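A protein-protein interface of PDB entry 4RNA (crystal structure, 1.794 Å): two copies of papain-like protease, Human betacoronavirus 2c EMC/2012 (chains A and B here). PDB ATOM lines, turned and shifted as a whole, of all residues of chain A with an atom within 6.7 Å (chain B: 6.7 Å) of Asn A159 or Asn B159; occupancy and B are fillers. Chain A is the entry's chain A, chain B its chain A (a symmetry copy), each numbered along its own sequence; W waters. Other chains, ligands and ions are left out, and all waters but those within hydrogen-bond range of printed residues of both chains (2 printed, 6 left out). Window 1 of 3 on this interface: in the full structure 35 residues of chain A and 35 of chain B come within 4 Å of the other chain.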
ATOM      1  N   ASP A  78     -18.867   5.693   8.374  1.00  0.00           N
ATOM      2  CA  ASP A  78     -19.838   4.995   9.212  1.00  0.00           C
ATOM      3  C   ASP A  78     -20.549   3.872   8.418  1.00  0.00           C
ATOM      4  O   ASP A  78     -20.542   3.861   7.186  1.00  0.00           O
ATOM      5  CB  ASP A  78     -20.905   5.967   9.753  1.00  0.00           C
ATOM      6  CG  ASP A  78     -22.034   6.205   8.794  1.00  0.00           C
ATOM      7  OD1 ASP A  78     -21.858   7.070   7.889  1.00  0.00           O
ATOM      8  OD2 ASP A  78     -23.135   5.559   8.946  1.00  0.00           O
ATOM      9  N   THR A  80     -23.362   3.113   7.690  1.00  0.00           N
ATOM     10  CA  THR A  80     -24.463   3.391   6.747  1.00  0.00           C
ATOM     11  C   THR A  80     -24.025   4.077   5.430  1.00  0.00           C
ATOM     12  O   THR A  80     -24.808   4.372   4.528  1.00  0.00           O
ATOM     13  CB  THR A  80     -25.514   4.323   7.390  1.00  0.00           C
ATOM     14  OG1 THR A  80     -25.010   5.693   7.504  1.00  0.00           O
ATOM     15  CG2 THR A  80     -26.044   3.727   8.826  1.00  0.00           C
ATOM     16  N   ARG A  84     -26.100   4.893   1.892  1.00  0.00           N
ATOM     17  CA  ARG A  84     -26.449   6.326   1.572  1.00  0.00           C
ATOM     18  C   ARG A  84     -25.849   6.854   0.259  1.00  0.00           C
ATOM     19  O   ARG A  84     -26.526   7.436  -0.546  1.00  0.00           O
ATOM     20  CB  ARG A  84     -26.147   7.266   2.750  1.00  0.00           C
ATOM     21  CG  ARG A  84     -27.019   6.974   3.999  1.00  0.00           C
ATOM     22  CD  ARG A  84     -26.695   7.898   5.207  1.00  0.00           C
ATOM     23  NE  ARG A  84     -25.267   7.810   5.650  1.00  0.00           N
ATOM     24  CZ  ARG A  84     -24.339   8.720   5.400  1.00  0.00           C
ATOM     25  NH1 ARG A  84     -24.583   9.785   4.621  1.00  0.00           N
ATOM     26  NH2 ARG A  84     -23.082   8.507   5.840  1.00  0.00           N
ATOM     27  N   LEU A 153     -21.169  11.954  -3.502  1.00  0.00           N
ATOM     28  CA  LEU A 153     -20.206  11.837  -2.439  1.00  0.00           C
ATOM     29  C   LEU A 153     -20.159  13.001  -1.421  1.00  0.00           C
ATOM     30  O   LEU A 153     -20.061  12.769  -0.211  1.00  0.00           O
ATOM     31  CB  LEU A 153     -18.822  11.634  -3.025  1.00  0.00           C
ATOM     32  CG  LEU A 153     -18.458  10.219  -3.517  1.00  0.00           C
ATOM     33  CD1 LEU A 153     -17.054  10.259  -4.096  1.00  0.00           C
ATOM     34  CD2 LEU A 153     -18.536   9.141  -2.435  1.00  0.00           C
ATOM     35  N   ILE A 154     -20.206  14.255  -1.904  1.00  0.00           N
ATOM     36  CA  ILE A 154     -20.282  15.407  -1.035  1.00  0.00           C
ATOM     37  C   ILE A 154     -21.494  15.226  -0.151  1.00  0.00           C
ATOM     38  O   ILE A 154     -21.390  15.434   1.055  1.00  0.00           O
ATOM     39  CB  ILE A 154     -20.383  16.743  -1.847  1.00  0.00           C
ATOM     40  CG1 ILE A 154     -19.067  17.073  -2.513  1.00  0.00           C
ATOM     41  CG2 ILE A 154     -20.891  17.907  -0.992  1.00  0.00           C
ATOM     42  CD1 ILE A 154     -19.245  18.338  -3.342  1.00  0.00           C
ATOM     43  N   MET A 155     -22.644  14.881  -0.717  1.00  0.00           N
ATOM     44  CA  MET A 155     -23.829  14.656   0.094  1.00  0.00           C
ATOM     45  C   MET A 155     -23.673  13.510   1.152  1.00  0.00           C
ATOM     46  O   MET A 155     -24.137  13.647   2.321  1.00  0.00           O
ATOM     47  CB  MET A 155     -25.023  14.402  -0.834  1.00  0.00           C
ATOM     48  CG  MET A 155     -25.422  15.678  -1.511  1.00  0.00           C
ATOM     49  SD  MET A 155     -26.758  15.308  -2.641  1.00  0.00           S
ATOM     50  CE  MET A 155     -28.147  15.586  -1.534  1.00  0.00           C
ATOM     51  N   ALA A 156     -22.992  12.420   0.766  1.00  0.00           N
ATOM     52  CA  ALA A 156     -22.797  11.266   1.652  1.00  0.00           C
ATOM     53  C   ALA A 156     -21.865  11.631   2.782  1.00  0.00           C
ATOM     54  O   ALA A 156     -22.231  11.486   3.978  1.00  0.00           O
ATOM     55  CB  ALA A 156     -22.324  10.026   0.867  1.00  0.00           C
ATOM     56  N   TYR A 157     -20.705  12.195   2.419  1.00  0.00           N
ATOM     57  CA  TYR A 157     -19.740  12.634   3.429  1.00  0.00           C
ATOM     58  C   TYR A 157     -20.324  13.795   4.285  1.00  0.00           C
ATOM     59  O   TYR A 157     -19.999  13.903   5.454  1.00  0.00           O
ATOM     60  CB  TYR A 157     -18.456  13.110   2.756  1.00  0.00           C
ATOM     61  CG  TYR A 157     -17.546  11.987   2.300  1.00  0.00           C
ATOM     62  CD1 TYR A 157     -16.972  11.080   3.232  1.00  0.00           C
ATOM     63  CD2 TYR A 157     -17.277  11.811   0.945  1.00  0.00           C
ATOM     64  CE1 TYR A 157     -16.154  10.027   2.808  1.00  0.00           C
ATOM     65  CE2 TYR A 157     -16.478  10.743   0.493  1.00  0.00           C
ATOM     66  CZ  TYR A 157     -15.901   9.877   1.428  1.00  0.00           C
ATOM     67  OH  TYR A 157     -15.110   8.865   0.998  1.00  0.00           O
ATOM     68  N   GLY A 158     -21.249  14.586   3.721  1.00  0.00           N
ATOM     69  CA  GLY A 158     -21.784  15.775   4.407  1.00  0.00           C
ATOM     70  C   GLY A 158     -23.053  15.479   5.225  1.00  0.00           C
ATOM     71  O   GLY A 158     -23.556  16.309   5.975  1.00  0.00           O
ATOM     72  N   ASN A 159     -23.550  14.258   5.079  1.00  0.00           N
ATOM     73  CA  ASN A 159     -24.711  13.772   5.747  1.00  0.00           C
ATOM     74  C   ASN A 159     -25.873  14.584   5.371  1.00  0.00           C
ATOM     75  O   ASN A 159     -26.663  14.896   6.237  1.00  0.00           O
ATOM     76  CB  ASN A 159     -24.531  13.829   7.263  1.00  0.00           C
ATOM     77  CG  ASN A 159     -23.527  12.833   7.739  1.00  0.00           C
ATOM     78  OD1 ASN A 159     -23.589  11.673   7.380  1.00  0.00           O
ATOM     79  ND2 ASN A 159     -22.587  13.275   8.556  1.00  0.00           N
ATOM     80  N   CYS A 160     -25.959  14.922   4.087  1.00  0.00           N
ATOM     81  CA  CYS A 160     -27.105  15.635   3.525  1.00  0.00           C
ATOM     82  C   CYS A 160     -28.204  14.646   3.248  1.00  0.00           C
ATOM     83  O   CYS A 160     -27.956  13.505   2.822  1.00  0.00           O
ATOM     84  CB  CYS A 160     -26.711  16.431   2.252  1.00  0.00           C
ATOM     85  SG  CYS A 160     -25.171  17.353   2.533  1.00  0.00           S
ATOM     86  N   THR A 161     -29.427  15.094   3.483  1.00  0.00           N
ATOM     87  CA  THR A 161     -30.596  14.259   3.304  1.00  0.00           C
ATOM     88  C   THR A 161     -31.151  14.822   2.029  1.00  0.00           C
ATOM     89  O   THR A 161     -31.336  16.036   1.918  1.00  0.00           O
ATOM     90  CB  THR A 161     -31.624  14.438   4.483  1.00  0.00           C
ATOM     91  OG1 THR A 161     -30.970  14.315   5.765  1.00  0.00           O
ATOM     92  CG2 THR A 161     -32.696  13.436   4.405  1.00  0.00           C
ATOM     93  N   ASP A 166     -29.655  22.746   3.463  1.00  0.00           N
ATOM     94  CA  ASP A 166     -28.477  22.468   4.247  1.00  0.00           C
ATOM     95  C   ASP A 166     -27.615  23.709   4.238  1.00  0.00           C
ATOM     96  O   ASP A 166     -27.939  24.699   3.582  1.00  0.00           O
ATOM     97  CB  ASP A 166     -27.733  21.228   3.718  1.00  0.00           C
ATOM     98  CG  ASP A 166     -27.071  20.429   4.836  1.00  0.00           C
ATOM     99  OD1 ASP A 166     -26.343  21.021   5.677  1.00  0.00           O
ATOM    100  OD2 ASP A 166     -27.338  19.206   4.870  1.00  0.00           O
ATOM    101  N   ARG A 170     -21.066  25.025   6.059  1.00  0.00           N
ATOM    102  CA  ARG A 170     -20.727  23.782   6.788  1.00  0.00           C
ATOM    103  C   ARG A 170     -20.159  22.800   5.788  1.00  0.00           C
ATOM    104  O   ARG A 170     -19.121  22.206   6.014  1.00  0.00           O
ATOM    105  CB  ARG A 170     -21.963  23.182   7.455  1.00  0.00           C
ATOM    106  CG  ARG A 170     -21.715  21.855   8.213  1.00  0.00           C
ATOM    107  CD  ARG A 170     -23.067  21.284   8.677  1.00  0.00           C
ATOM    108  NE  ARG A 170     -23.759  20.547   7.623  1.00  0.00           N
ATOM    109  CZ  ARG A 170     -23.381  19.372   7.091  1.00  0.00           C
ATOM    110  NH1 ARG A 170     -22.216  18.699   7.382  1.00  0.00           N
ATOM    111  NH2 ARG A 170     -24.149  18.893   6.168  1.00  0.00           N
ATOM    112  N   LEU A 171     -20.848  22.621   4.674  1.00  0.00           N
ATOM    113  CA  LEU A 171     -20.358  21.644   3.649  1.00  0.00           C
ATOM    114  C   LEU A 171     -19.043  21.969   3.031  1.00  0.00           C
ATOM    115  O   LEU A 171     -18.156  21.055   2.829  1.00  0.00           O
ATOM    116  CB  LEU A 171     -21.421  21.488   2.545  1.00  0.00           C
ATOM    117  CG  LEU A 171     -22.194  20.191   2.432  1.00  0.00           C
ATOM    118  CD1 LEU A 171     -21.373  18.902   2.703  1.00  0.00           C
ATOM    119  CD2 LEU A 171     -23.347  20.332   3.404  1.00  0.00           C
ATOM    120  N   THR A 174     -16.481  20.917   5.542  1.00  0.00           N
ATOM    121  CA  THR A 174     -16.332  19.480   5.614  1.00  0.00           C
ATOM    122  C   THR A 174     -15.692  18.849   4.408  1.00  0.00           C
ATOM    123  O   THR A 174     -14.925  17.874   4.534  1.00  0.00           O
ATOM    124  CB  THR A 174     -17.684  18.736   5.788  1.00  0.00           C
ATOM    125  OG1 THR A 174     -18.569  19.147   4.751  1.00  0.00           O
ATOM    126  CG2 THR A 174     -18.316  19.082   7.026  1.00  0.00           C
ATOM    127  N   ASP B  78     -16.008  21.086  13.313  1.00  0.00           N
ATOM    128  CA  ASP B  78     -15.882  22.028  12.204  1.00  0.00           C
ATOM    129  C   ASP B  78     -16.253  23.464  12.651  1.00  0.00           C
ATOM    130  O   ASP B  78     -16.908  23.661  13.676  1.00  0.00           O
ATOM    131  CB  ASP B  78     -16.795  21.628  11.029  1.00  0.00           C
ATOM    132  CG  ASP B  78     -18.204  22.122  11.175  1.00  0.00           C
ATOM    133  OD1 ASP B  78     -18.994  21.434  11.884  1.00  0.00           O
ATOM    134  OD2 ASP B  78     -18.564  23.189  10.556  1.00  0.00           O
ATOM    135  N   THR B  80     -18.208  25.598  11.852  1.00  0.00           N
ATOM    136  CA  THR B  80     -19.609  26.042  11.994  1.00  0.00           C
ATOM    137  C   THR B  80     -20.353  25.444  13.213  1.00  0.00           C
ATOM    138  O   THR B  80     -21.522  25.712  13.490  1.00  0.00           O
ATOM    139  CB  THR B  80     -20.436  25.652  10.749  1.00  0.00           C
ATOM    140  OG1 THR B  80     -20.695  24.211  10.714  1.00  0.00           O
ATOM    141  CG2 THR B  80     -19.734  26.198   9.368  1.00  0.00           C
ATOM    142  N   ARG B  84     -24.087  26.304  14.890  1.00  0.00           N
ATOM    143  CA  ARG B  84     -25.196  25.293  14.743  1.00  0.00           C
ATOM    144  C   ARG B  84     -25.751  24.751  16.070  1.00  0.00           C
ATOM    145  O   ARG B  84     -26.934  24.705  16.279  1.00  0.00           O
ATOM    146  CB  ARG B  84     -24.810  24.154  13.785  1.00  0.00           C
ATOM    147  CG  ARG B  84     -24.592  24.634  12.326  1.00  0.00           C
ATOM    148  CD  ARG B  84     -24.166  23.494  11.359  1.00  0.00           C
ATOM    149  NE  ARG B  84     -22.903  22.806  11.778  1.00  0.00           N
ATOM    150  CZ  ARG B  84     -22.844  21.611  12.345  1.00  0.00           C
ATOM    151  NH1 ARG B  84     -23.951  20.935  12.690  1.00  0.00           N
ATOM    152  NH2 ARG B  84     -21.640  21.114  12.693  1.00  0.00           N
ATOM    153  N   LEU B 153     -27.051  18.676  20.914  1.00  0.00           N
ATOM    154  CA  LEU B 153     -25.759  18.142  20.573  1.00  0.00           C
ATOM    155  C   LEU B 153     -25.743  16.960  19.575  1.00  0.00           C
ATOM    156  O   LEU B 153     -24.909  16.923  18.664  1.00  0.00           O
ATOM    157  CB  LEU B 153     -25.027  17.734  21.837  1.00  0.00           C
ATOM    158  CG  LEU B 153     -24.354  18.850  22.662  1.00  0.00           C
ATOM    159  CD1 LEU B 153     -23.723  18.223  23.892  1.00  0.00           C
ATOM    160  CD2 LEU B 153     -23.298  19.646  21.893  1.00  0.00           C
ATOM    161  N   ILE B 154     -26.646  15.980  19.754  1.00  0.00           N
ATOM    162  CA  ILE B 154     -26.790  14.891  18.815  1.00  0.00           C
ATOM    163  C   ILE B 154     -27.057  15.499  17.457  1.00  0.00           C
ATOM    164  O   ILE B 154     -26.434  15.082  16.484  1.00  0.00           O
ATOM    165  CB  ILE B 154     -27.948  13.919  19.224  1.00  0.00           C
ATOM    166  CG1 ILE B 154     -27.565  13.099  20.434  1.00  0.00           C
ATOM    167  CG2 ILE B 154     -28.400  13.032  18.060  1.00  0.00           C
ATOM    168  CD1 ILE B 154     -28.750  12.227  20.826  1.00  0.00           C
ATOM    169  N   MET B 155     -27.984  16.443  17.357  1.00  0.00           N
ATOM    170  CA  MET B 155     -28.250  17.087  16.082  1.00  0.00           C
ATOM    171  C   MET B 155     -27.013  17.831  15.470  1.00  0.00           C
ATOM    172  O   MET B 155     -26.767  17.757  14.232  1.00  0.00           O
ATOM    173  CB  MET B 155     -29.447  18.031  16.244  1.00  0.00           C
ATOM    174  CG  MET B 155     -30.708  17.234  16.389  1.00  0.00           C
ATOM    175  SD  MET B 155     -32.056  18.378  16.659  1.00  0.00           S
ATOM    176  CE  MET B 155     -32.546  18.642  14.951  1.00  0.00           C
ATOM    177  N   ALA B 156     -26.224  18.497  16.327  1.00  0.00           N
ATOM    178  CA  ALA B 156     -25.050  19.256  15.880  1.00  0.00           C
ATOM    179  C   ALA B 156     -23.977  18.313  15.392  1.00  0.00           C
ATOM    180  O   ALA B 156     -23.512  18.430  14.228  1.00  0.00           O
ATOM    181  CB  ALA B 156     -24.546  20.214  16.977  1.00  0.00           C
ATOM    182  N   TYR B 157     -23.651  17.320  16.231  1.00  0.00           N
ATOM    183  CA  TYR B 157     -22.657  16.315  15.849  1.00  0.00           C
ATOM    184  C   TYR B 157     -23.160  15.469  14.644  1.00  0.00           C
ATOM    185  O   TYR B 157     -22.357  15.035  13.836  1.00  0.00           O
ATOM    186  CB  TYR B 157     -22.370  15.387  17.025  1.00  0.00           C
ATOM    187  CG  TYR B 157     -21.445  15.981  18.069  1.00  0.00           C
ATOM    188  CD1 TYR B 157     -20.106  16.335  17.750  1.00  0.00           C
ATOM    189  CD2 TYR B 157     -21.907  16.212  19.362  1.00  0.00           C
ATOM    190  CE1 TYR B 157     -19.262  16.909  18.706  1.00  0.00           C
ATOM    191  CE2 TYR B 157     -21.083  16.811  20.334  1.00  0.00           C
ATOM    192  CZ  TYR B 157     -19.761  17.130  20.007  1.00  0.00           C
ATOM    193  OH  TYR B 157     -18.957  17.681  20.948  1.00  0.00           O
ATOM    194  N   GLY B 158     -24.484  15.326  14.487  1.00  0.00           N
ATOM    195  CA  GLY B 158     -25.060  14.458  13.446  1.00  0.00           C
ATOM    196  C   GLY B 158     -25.345  15.203  12.130  1.00  0.00           C
ATOM    197  O   GLY B 158     -25.689  14.616  11.108  1.00  0.00           O
ATOM    198  N   ASN B 159     -25.171  16.516  12.172  1.00  0.00           N
ATOM    199  CA  ASN B 159     -25.370  17.395  11.069  1.00  0.00           C
ATOM    200  C   ASN B 159     -26.766  17.321  10.625  1.00  0.00           C
ATOM    201  O   ASN B 159     -26.993  17.302   9.434  1.00  0.00           O
ATOM    202  CB  ASN B 159     -24.455  17.022   9.903  1.00  0.00           C
ATOM    203  CG  ASN B 159     -23.024  17.315  10.208  1.00  0.00           C
ATOM    204  OD1 ASN B 159     -22.697  18.399  10.652  1.00  0.00           O
ATOM    205  ND2 ASN B 159     -22.153  16.351   9.971  1.00  0.00           N
ATOM    206  N   CYS B 160     -27.683  17.272  11.588  1.00  0.00           N
ATOM    207  CA  CYS B 160     -29.121  17.305  11.322  1.00  0.00           C
ATOM    208  C   CYS B 160     -29.544  18.733  11.111  1.00  0.00           C
ATOM    209  O   CYS B 160     -29.049  19.660  11.776  1.00  0.00           O
ATOM    210  CB  CYS B 160     -29.926  16.627  12.464  1.00  0.00           C
ATOM    211  SG  CYS B 160     -29.165  15.041  12.920  1.00  0.00           S
ATOM    212  N   THR B 161     -30.474  18.906  10.187  1.00  0.00           N
ATOM    213  CA  THR B 161     -30.968  20.220   9.834  1.00  0.00           C
ATOM    214  C   THR B 161     -32.311  20.205  10.500  1.00  0.00           C
ATOM    215  O   THR B 161     -33.089  19.269  10.303  1.00  0.00           O
ATOM    216  CB  THR B 161     -31.123  20.383   8.275  1.00  0.00           C
ATOM    217  OG1 THR B 161     -29.922  19.971   7.587  1.00  0.00           O
ATOM    218  CG2 THR B 161     -31.414  21.779   7.916  1.00  0.00           C
ATOM    219  N   ASP B 166     -34.365  12.442   8.887  1.00  0.00           N
ATOM    220  CA  ASP B 166     -32.998  11.986   8.918  1.00  0.00           C
ATOM    221  C   ASP B 166     -33.015  10.502   9.199  1.00  0.00           C
ATOM    222  O   ASP B 166     -34.074   9.910   9.411  1.00  0.00           O
ATOM    223  CB  ASP B 166     -32.170  12.773   9.952  1.00  0.00           C
ATOM    224  CG  ASP B 166     -30.722  12.963   9.510  1.00  0.00           C
ATOM    225  OD1 ASP B 166     -30.056  11.969   9.115  1.00  0.00           O
ATOM    226  OD2 ASP B 166     -30.292  14.139   9.528  1.00  0.00           O
ATOM    227  N   ARG B 170     -28.176   5.899  11.026  1.00  0.00           N
ATOM    228  CA  ARG B 170     -26.944   6.689  10.800  1.00  0.00           C
ATOM    229  C   ARG B 170     -26.616   7.413  12.087  1.00  0.00           C
ATOM    230  O   ARG B 170     -25.493   7.383  12.554  1.00  0.00           O
ATOM    231  CB  ARG B 170     -27.140   7.703   9.674  1.00  0.00           C
ATOM    232  CG  ARG B 170     -25.914   8.605   9.389  1.00  0.00           C
ATOM    233  CD  ARG B 170     -26.314   9.681   8.363  1.00  0.00           C
ATOM    234  NE  ARG B 170     -27.000  10.816   8.976  1.00  0.00           N
ATOM    235  CZ  ARG B 170     -26.456  11.725   9.803  1.00  0.00           C
ATOM    236  NH1 ARG B 170     -25.172  11.691  10.296  1.00  0.00           N
ATOM    237  NH2 ARG B 170     -27.249  12.653  10.226  1.00  0.00           N
ATOM    238  N   LEU B 171     -27.604   8.076  12.664  1.00  0.00           N
ATOM    239  CA  LEU B 171     -27.346   8.837  13.929  1.00  0.00           C
ATOM    240  C   LEU B 171     -26.935   8.014  15.099  1.00  0.00           C
ATOM    241  O   LEU B 171     -25.991   8.400  15.888  1.00  0.00           O
ATOM    242  CB  LEU B 171     -28.596   9.661  14.291  1.00  0.00           C
ATOM    243  CG  LEU B 171     -28.557  11.169  14.169  1.00  0.00           C
ATOM    244  CD1 LEU B 171     -27.220  11.835  14.590  1.00  0.00           C
ATOM    245  CD2 LEU B 171     -28.892  11.457  12.720  1.00  0.00           C
ATOM    246  N   THR B 174     -23.308   7.280  14.571  1.00  0.00           N
ATOM    247  CA  THR B 174     -22.467   8.432  14.816  1.00  0.00           C
ATOM    248  C   THR B 174     -22.372   8.851  16.258  1.00  0.00           C
ATOM    249  O   THR B 174     -21.304   9.297  16.720  1.00  0.00           O
ATOM    250  CB  THR B 174     -22.940   9.702  14.057  1.00  0.00           C
ATOM    251  OG1 THR B 174     -24.307   9.941  14.373  1.00  0.00           O
ATOM    252  CG2 THR B 174     -22.874   9.519  12.638  1.00  0.00           C
HETATM  253  O   HOH W   1     -22.101  12.842  11.566  1.00  0.00           O
HETATM  254  O   HOH W   2     -19.982  16.017   7.812  1.00  0.00           O
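ND2 of Asn A159 sits close to ND2 of Asn B159, 3.4 Å away.
NH1 of Arg B170 lies close to OD1 of Asn A159, 3.3 Å away.
The guanidinium group (NH1) of Arg A170 sits close to the side-chain amide oxygen (OD1) of Asn B159 (3.3 Å).
N of Thr A80 lies within hydrogen-bond range of OD2 of Asp A78 (2.8 Å).
The side-chain carboxylate (OD1) of Asp A78 is in salt-bridge range of the guanidinium group (NH2) of Arg A84, at 2.8 Å.
The backbone carbonyl oxygen (O) of Gly A158 lies within hydrogen-bond range of the guanidinium group (NH2) of Arg A170 (2.7 Å).
The side-chain carboxylate (OD2) of Asp A166 is in hydrogen-bond range of the side-chain sulfur (SG) of Cys A160, 3.7 Å away.
The backbone carbonyl oxygen (O) of Arg A170 sits at hydrogen-bond distance from the side-chain hydroxyl (OG1) of Thr A174 (3.4 Å).
The guanidinium group (NH1) of Arg B84 lies within hydrogen-bond range of the side-chain amide oxygen (OD1) of Asn B159.
Among the printed residues, pairs that only touch across the chains: Thr A80 with Arg B170, Arg A84 with Arg B170, Thr A161 with Asp B166, Asp A166 with Thr B161, Arg A170 with Thr B80 and Arg A170 with Arg B84.
Of chain B, only Asn B159 and Arg B170 come within 4 Å of Asn A159.
Of the printed residues of chain A, Asn B159 touches Asn A159 (3.4 Å) and Arg A170 (3.2 Å).
Printed residues of chain A within 4 Å of Arg B170: Thr A80, Arg A84 and Asn A159.
Of the printed residues of chain A, Asp B166 touches Thr A161.
Printed residues of chain B within 4 Å of Asp A166: Thr B161.
Printed residues of chain A within 4 Å of Arg B84: Arg A170.
Gly A158 touches none of the printed residues of chain B.
Cys B160 touches none of the printed residues of chain A.
The nearest residue of chain B that does not touch Asn A159 is Gly B158 (4.1 Å).
The nearest residue of chain A that does not touch Asn B159 is Gly A158 (4.1 Å).
The nearest printed residue of chain A that does not touch Thr B161 is Thr A161 (6.0 Å).
Of the 16 printed residues of chain A, 6 touch a printed residue of chain B.
Along chain A the printed residues that touch a printed residue of chain B span positions 80 to 170.
Of the 16 printed residues of chain B, 6 touch a printed residue of chain A.
Among the printed residues, 9 pairs touch across the chains.
Arg A84 touches Arg B170, and with the chains exchanged Arg A170 touches Arg B84.
Asn B159 touches its own counterpart, Asn A159.
Asn A159 touches Arg B170, and with the chains exchanged Arg A170 touches Asn B159.
Thr A161 touches Asp B166, and with the chains exchanged Asp A166 touches Thr B161.
Positions printed for both chains: 78, 80, 84, 153, 154, 155, 156, 157, 158, 159, 160, 161, 166, 170, 171 and 174.
Of the 9 pairs that touch across the chains among the printed residues, 9 have their exchanged pair printed and touching as well.
Water W1 bridges the side-chain amide nitrogen of Asn A159 and the backbone carbonyl oxygen of Tyr B157.
Water W2 bridges the side-chain amide nitrogen (ND2) of Asn B159 (3.1 Å) and the backbone carbonyl oxygen (O) of Tyr A157 (3.2 Å).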
